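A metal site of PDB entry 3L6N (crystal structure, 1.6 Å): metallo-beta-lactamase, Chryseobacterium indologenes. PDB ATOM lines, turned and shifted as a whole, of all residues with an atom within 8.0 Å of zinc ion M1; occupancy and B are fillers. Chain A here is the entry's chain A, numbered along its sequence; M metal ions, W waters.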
ATOM      1  N   SER A  30      37.484 -26.009 -21.792  1.00  0.00           N
ATOM      2  CA  SER A  30      36.995 -24.822 -22.441  1.00  0.00           C
ATOM      3  C   SER A  30      35.568 -24.554 -21.984  1.00  0.00           C
ATOM      4  O   SER A  30      34.819 -25.494 -21.654  1.00  0.00           O
ATOM      5  CB  SER A  30      37.028 -25.015 -23.965  1.00  0.00           C
ATOM      6  OG  SER A  30      36.979 -23.783 -24.648  1.00  0.00           O
ATOM      7  N   ALA A  31      35.212 -23.281 -21.930  1.00  0.00           N
ATOM      8  CA  ALA A  31      33.826 -22.883 -21.701  1.00  0.00           C
ATOM      9  C   ALA A  31      33.474 -21.857 -22.750  1.00  0.00           C
ATOM     10  O   ALA A  31      34.263 -20.954 -23.022  1.00  0.00           O
ATOM     11  CB  ALA A  31      33.648 -22.285 -20.303  1.00  0.00           C
ATOM     12  N   ASN A  32      32.285 -21.987 -23.333  1.00  0.00           N
ATOM     13  CA  ASN A  32      31.785 -21.023 -24.307  1.00  0.00           C
ATOM     14  C   ASN A  32      30.838 -20.042 -23.664  1.00  0.00           C
ATOM     15  O   ASN A  32      29.876 -20.435 -23.005  1.00  0.00           O
ATOM     16  CB  ASN A  32      31.070 -21.757 -25.435  1.00  0.00           C
ATOM     17  CG  ASN A  32      31.924 -22.826 -26.057  1.00  0.00           C
ATOM     18  OD1 ASN A  32      33.057 -22.563 -26.461  1.00  0.00           O
ATOM     19  ND2 ASN A  32      31.393 -24.042 -26.097  1.00  0.00           N
ATOM     20  N   ASP A  46      27.637 -14.657 -19.276  1.00  0.00           N
ATOM     21  CA  ASP A  46      28.639 -15.433 -18.536  1.00  0.00           C
ATOM     22  C   ASP A  46      30.018 -14.831 -18.694  1.00  0.00           C
ATOM     23  O   ASP A  46      30.276 -14.046 -19.598  1.00  0.00           O
ATOM     24  CB  ASP A  46      28.577 -16.919 -18.884  1.00  0.00           C
ATOM     25  CG  ASP A  46      27.214 -17.488 -18.579  1.00  0.00           C
ATOM     26  OD1 ASP A  46      26.731 -17.207 -17.475  1.00  0.00           O
ATOM     27  OD2 ASP A  46      26.647 -18.207 -19.440  1.00  0.00           O
ATOM     28  N   TRP A  49      36.157 -18.112 -17.296  1.00  0.00           N
ATOM     29  CA  TRP A  49      36.261 -19.184 -16.304  1.00  0.00           C
ATOM     30  C   TRP A  49      37.227 -18.818 -15.180  1.00  0.00           C
ATOM     31  O   TRP A  49      36.961 -19.094 -14.005  1.00  0.00           O
ATOM     32  CB  TRP A  49      36.679 -20.497 -16.965  1.00  0.00           C
ATOM     33  CG  TRP A  49      36.134 -21.739 -16.279  1.00  0.00           C
ATOM     34  CD1 TRP A  49      35.697 -21.859 -14.979  1.00  0.00           C
ATOM     35  CD2 TRP A  49      35.957 -23.032 -16.873  1.00  0.00           C
ATOM     36  NE1 TRP A  49      35.267 -23.144 -14.733  1.00  0.00           N
ATOM     37  CE2 TRP A  49      35.417 -23.879 -15.878  1.00  0.00           C
ATOM     38  CE3 TRP A  49      36.229 -23.550 -18.150  1.00  0.00           C
ATOM     39  CZ2 TRP A  49      35.106 -25.229 -16.133  1.00  0.00           C
ATOM     40  CZ3 TRP A  49      35.903 -24.909 -18.403  1.00  0.00           C
ATOM     41  CH2 TRP A  49      35.362 -25.721 -17.389  1.00  0.00           C
ATOM     42  N   THR A  75      24.043 -17.256 -16.577  1.00  0.00           N
ATOM     43  CA  THR A  75      23.101 -18.306 -16.964  1.00  0.00           C
ATOM     44  C   THR A  75      22.986 -19.451 -15.946  1.00  0.00           C
ATOM     45  O   THR A  75      22.156 -20.354 -16.118  1.00  0.00           O
ATOM     46  CB  THR A  75      23.308 -18.848 -18.403  1.00  0.00           C
ATOM     47  OG1 THR A  75      24.566 -19.525 -18.477  1.00  0.00           O
ATOM     48  CG2 THR A  75      23.255 -17.718 -19.427  1.00  0.00           C
ATOM     49  N   HIS A  76      23.830 -19.424 -14.930  1.00  0.00           N
ATOM     50  CA  HIS A  76      23.608 -20.119 -13.642  1.00  0.00           C
ATOM     51  C   HIS A  76      24.718 -19.734 -12.656  1.00  0.00           C
ATOM     52  O   HIS A  76      25.531 -18.840 -12.960  1.00  0.00           O
ATOM     53  CB  HIS A  76      23.348 -21.655 -13.748  1.00  0.00           C
ATOM     54  CG  HIS A  76      24.486 -22.483 -14.287  1.00  0.00           C
ATOM     55  ND1 HIS A  76      24.737 -22.616 -15.636  1.00  0.00           N
ATOM     56  CD2 HIS A  76      25.345 -23.314 -13.649  1.00  0.00           C
ATOM     57  CE1 HIS A  76      25.760 -23.440 -15.806  1.00  0.00           C
ATOM     58  NE2 HIS A  76      26.149 -23.879 -14.619  1.00  0.00           N
ATOM     59  N   HIS A  78      27.394 -21.240 -11.282  1.00  0.00           N
ATOM     60  CA  HIS A  78      28.733 -21.833 -11.274  1.00  0.00           C
ATOM     61  C   HIS A  78      29.836 -20.883 -11.719  1.00  0.00           C
ATOM     62  O   HIS A  78      29.590 -19.841 -12.335  1.00  0.00           O
ATOM     63  CB  HIS A  78      28.759 -23.086 -12.151  1.00  0.00           C
ATOM     64  CG  HIS A  78      28.059 -24.262 -11.543  1.00  0.00           C
ATOM     65  ND1 HIS A  78      27.643 -25.351 -12.293  1.00  0.00           N
ATOM     66  CD2 HIS A  78      27.736 -24.545 -10.262  1.00  0.00           C
ATOM     67  CE1 HIS A  78      27.100 -26.246 -11.485  1.00  0.00           C
ATOM     68  NE2 HIS A  78      27.126 -25.772 -10.254  1.00  0.00           N
ATOM     69  N   ASP A  79      31.067 -21.249 -11.384  1.00  0.00           N
ATOM     70  CA  ASP A  79      32.249 -20.394 -11.642  1.00  0.00           C
ATOM     71  C   ASP A  79      32.460 -19.981 -13.093  1.00  0.00           C
ATOM     72  O   ASP A  79      32.982 -18.890 -13.359  1.00  0.00           O
ATOM     73  CB  ASP A  79      33.521 -21.098 -11.187  1.00  0.00           C
ATOM     74  CG  ASP A  79      33.627 -21.259  -9.682  1.00  0.00           C
ATOM     75  OD1 ASP A  79      34.549 -21.984  -9.264  1.00  0.00           O
ATOM     76  OD2 ASP A  79      32.828 -20.679  -8.921  1.00  0.00           O
ATOM     77  N   ASP A  80      32.067 -20.853 -14.029  1.00  0.00           N
ATOM     78  CA  ASP A  80      32.204 -20.593 -15.462  1.00  0.00           C
ATOM     79  C   ASP A  80      31.027 -19.781 -16.023  1.00  0.00           C
ATOM     80  O   ASP A  80      30.950 -19.559 -17.225  1.00  0.00           O
ATOM     81  CB  ASP A  80      32.372 -21.913 -16.256  1.00  0.00           C
ATOM     82  CG  ASP A  80      31.198 -22.854 -16.092  1.00  0.00           C
ATOM     83  OD1 ASP A  80      30.770 -23.115 -14.952  1.00  0.00           O
ATOM     84  OD2 ASP A  80      30.701 -23.373 -17.130  1.00  0.00           O
ATOM     85  N   ARG A  81      30.155 -19.321 -15.128  1.00  0.00           N
ATOM     86  CA  ARG A  81      28.931 -18.636 -15.537  1.00  0.00           C
ATOM     87  C   ARG A  81      28.834 -17.305 -14.805  1.00  0.00           C
ATOM     88  O   ARG A  81      29.337 -16.293 -15.295  1.00  0.00           O
ATOM     89  CB  ARG A  81      27.720 -19.542 -15.284  1.00  0.00           C
ATOM     90  CG  ARG A  81      27.820 -20.933 -15.927  1.00  0.00           C
ATOM     91  CD  ARG A  81      27.414 -20.932 -17.391  1.00  0.00           C
ATOM     92  NE  ARG A  81      28.457 -20.420 -18.278  1.00  0.00           N
ATOM     93  CZ  ARG A  81      28.439 -20.554 -19.595  1.00  0.00           C
ATOM     94  NH1 ARG A  81      27.422 -21.168 -20.183  1.00  0.00           N
ATOM     95  NH2 ARG A  81      29.415 -20.052 -20.332  1.00  0.00           N
ATOM     96  N   HIS A 139      21.211 -29.428 -16.133  1.00  0.00           N
ATOM     97  CA  HIS A 139      22.580 -29.365 -15.647  1.00  0.00           C
ATOM     98  C   HIS A 139      22.610 -28.875 -14.186  1.00  0.00           C
ATOM     99  O   HIS A 139      23.374 -29.386 -13.383  1.00  0.00           O
ATOM    100  CB  HIS A 139      23.410 -28.449 -16.542  1.00  0.00           C
ATOM    101  CG  HIS A 139      24.727 -28.042 -15.944  1.00  0.00           C
ATOM    102  ND1 HIS A 139      25.800 -28.897 -15.829  1.00  0.00           N
ATOM    103  CD2 HIS A 139      25.122 -26.864 -15.410  1.00  0.00           C
ATOM    104  CE1 HIS A 139      26.808 -28.259 -15.256  1.00  0.00           C
ATOM    105  NE2 HIS A 139      26.418 -27.021 -14.991  1.00  0.00           N
ATOM    106  N   THR A 140      21.801 -27.857 -13.891  1.00  0.00           N
ATOM    107  CA  THR A 140      21.518 -27.432 -12.524  1.00  0.00           C
ATOM    108  C   THR A 140      20.035 -27.086 -12.402  1.00  0.00           C
ATOM    109  O   THR A 140      19.303 -27.094 -13.397  1.00  0.00           O
ATOM    110  CB  THR A 140      22.316 -26.174 -12.154  1.00  0.00           C
ATOM    111  OG1 THR A 140      22.055 -25.165 -13.138  1.00  0.00           O
ATOM    112  CG2 THR A 140      23.813 -26.465 -12.070  1.00  0.00           C
ATOM    113  N   GLY A 157      24.010 -22.661 -22.953  1.00  0.00           N
ATOM    114  CA  GLY A 157      24.764 -22.840 -21.724  1.00  0.00           C
ATOM    115  C   GLY A 157      24.982 -24.314 -21.424  1.00  0.00           C
ATOM    116  O   GLY A 157      24.912 -25.175 -22.316  1.00  0.00           O
ATOM    117  N   CYS A 158      25.177 -24.621 -20.159  1.00  0.00           N
ATOM    118  CA  CYS A 158      25.639 -25.935 -19.788  1.00  0.00           C
ATOM    119  C   CYS A 158      24.489 -26.960 -19.747  1.00  0.00           C
ATOM    120  O   CYS A 158      24.721 -28.154 -19.577  1.00  0.00           O
ATOM    121  CB  CYS A 158      26.456 -25.838 -18.499  1.00  0.00           C
ATOM    122  SG  CYS A 158      27.646 -24.435 -18.605  1.00  0.00           S
ATOM    123  N   LEU A 159      23.267 -26.475 -19.950  1.00  0.00           N
ATOM    124  CA  LEU A 159      22.102 -27.340 -20.180  1.00  0.00           C
ATOM    125  C   LEU A 159      22.296 -28.149 -21.470  1.00  0.00           C
ATOM    126  O   LEU A 159      21.833 -29.285 -21.582  1.00  0.00           O
ATOM    127  CB  LEU A 159      20.848 -26.467 -20.287  1.00  0.00           C
ATOM    128  CG  LEU A 159      19.506 -27.126 -20.647  1.00  0.00           C
ATOM    129  CD1 LEU A 159      19.077 -28.106 -19.533  1.00  0.00           C
ATOM    130  CD2 LEU A 159      18.462 -26.056 -20.873  1.00  0.00           C
ATOM    131  N   VAL A 160      23.004 -27.558 -22.440  1.00  0.00           N
ATOM    132  CA  VAL A 160      23.275 -28.216 -23.711  1.00  0.00           C
ATOM    133  C   VAL A 160      24.716 -28.694 -23.767  1.00  0.00           C
ATOM    134  O   VAL A 160      25.674 -27.915 -23.660  1.00  0.00           O
ATOM    135  CB  VAL A 160      22.995 -27.275 -24.899  1.00  0.00           C
ATOM    136  CG1 VAL A 160      23.276 -27.999 -26.239  1.00  0.00           C
ATOM    137  CG2 VAL A 160      21.556 -26.767 -24.850  1.00  0.00           C
ATOM    138  N   LYS A 161      24.870 -30.004 -23.927  1.00  0.00           N
ATOM    139  CA  LYS A 161      26.180 -30.617 -24.137  1.00  0.00           C
ATOM    140  C   LYS A 161      26.618 -30.492 -25.593  1.00  0.00           C
ATOM    141  O   LYS A 161      25.785 -30.514 -26.492  1.00  0.00           O
ATOM    142  CB  LYS A 161      26.135 -32.111 -23.763  1.00  0.00           C
ATOM    143  CG  LYS A 161      25.673 -32.396 -22.334  1.00  0.00           C
ATOM    144  CD  LYS A 161      26.587 -31.760 -21.299  1.00  0.00           C
ATOM    145  CE  LYS A 161      28.003 -32.288 -21.382  1.00  0.00           C
ATOM    146  NZ  LYS A 161      28.956 -31.524 -20.516  1.00  0.00           N
ATOM    147  N   TYR A 170      30.067 -32.417 -15.032  1.00  0.00           N
ATOM    148  CA  TYR A 170      29.751 -32.250 -13.617  1.00  0.00           C
ATOM    149  C   TYR A 170      28.251 -32.356 -13.364  1.00  0.00           C
ATOM    150  O   TYR A 170      27.483 -31.486 -13.783  1.00  0.00           O
ATOM    151  CB  TYR A 170      30.284 -30.903 -13.112  1.00  0.00           C
ATOM    152  CG  TYR A 170      29.991 -30.630 -11.664  1.00  0.00           C
ATOM    153  CD1 TYR A 170      30.683 -31.297 -10.638  1.00  0.00           C
ATOM    154  CD2 TYR A 170      29.024 -29.698 -11.289  1.00  0.00           C
ATOM    155  CE1 TYR A 170      30.410 -31.030  -9.296  1.00  0.00           C
ATOM    156  CE2 TYR A 170      28.739 -29.436  -9.954  1.00  0.00           C
ATOM    157  CZ  TYR A 170      29.437 -30.106  -8.964  1.00  0.00           C
ATOM    158  OH  TYR A 170      29.146 -29.836  -7.639  1.00  0.00           O
ATOM    159  N   PRO A 198      26.564 -24.653 -26.998  1.00  0.00           N
ATOM    160  CA  PRO A 198      26.732 -25.443 -25.772  1.00  0.00           C
ATOM    161  C   PRO A 198      27.705 -24.776 -24.806  1.00  0.00           C
ATOM    162  O   PRO A 198      28.610 -24.040 -25.222  1.00  0.00           O
ATOM    163  CB  PRO A 198      27.317 -26.758 -26.291  1.00  0.00           C
ATOM    164  CG  PRO A 198      28.148 -26.363 -27.492  1.00  0.00           C
ATOM    165  CD  PRO A 198      27.434 -25.139 -28.092  1.00  0.00           C
ATOM    166  N   GLY A 199      27.522 -25.030 -23.511  1.00  0.00           N
ATOM    167  CA  GLY A 199      28.335 -24.376 -22.484  1.00  0.00           C
ATOM    168  C   GLY A 199      29.825 -24.692 -22.526  1.00  0.00           C
ATOM    169  O   GLY A 199      30.644 -23.831 -22.212  1.00  0.00           O
ATOM    170  N   HIS A 200      30.154 -25.922 -22.909  1.00  0.00           N
ATOM    171  CA  HIS A 200      31.540 -26.394 -22.899  1.00  0.00           C
ATOM    172  C   HIS A 200      31.901 -27.090 -24.202  1.00  0.00           C
ATOM    173  O   HIS A 200      31.017 -27.567 -24.915  1.00  0.00           O
ATOM    174  CB  HIS A 200      31.750 -27.367 -21.746  1.00  0.00           C
ATOM    175  CG  HIS A 200      31.542 -26.757 -20.391  1.00  0.00           C
ATOM    176  ND1 HIS A 200      32.542 -26.086 -19.717  1.00  0.00           N
ATOM    177  CD2 HIS A 200      30.452 -26.733 -19.588  1.00  0.00           C
ATOM    178  CE1 HIS A 200      32.064 -25.675 -18.550  1.00  0.00           C
ATOM    179  NE2 HIS A 200      30.809 -26.046 -18.454  1.00  0.00           N
HETATM  180 ZN    ZN M   1      29.383 -24.929 -17.336  1.00  0.00          ZN
HETATM  181 ZN    ZN M   2      27.471 -25.471 -14.289  1.00  0.00          ZN
HETATM  182  O   HOH W   1      29.064 -25.120 -15.293  1.00  0.00           O
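Along chain A the residues within 4 Å of zinc ion M1 span positions 80 to 200.
Zinc ion M1 is bound by the side-chain carboxylate of Asp 80 (2.0 Å), water W1 (2.1 Å), a ring nitrogen (NE2) of His 200 (2.1 Å) and the side-chain sulfur of Cys 158 (2.2 Å).
The side-chain carboxylate (OD2) of Asp 80 lies close to the guanidinium group (NE) of Arg 81 (3.9 Å). The backbone carbonyl oxygen (O) of Ser 30 lies within hydrogen-bond range of a ring nitrogen (ND1) of His 200 (3.0 Å). The side-chain sulfur of Cys 158 sits close to the guanidinium group of Arg 81, 3.6 Å away.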
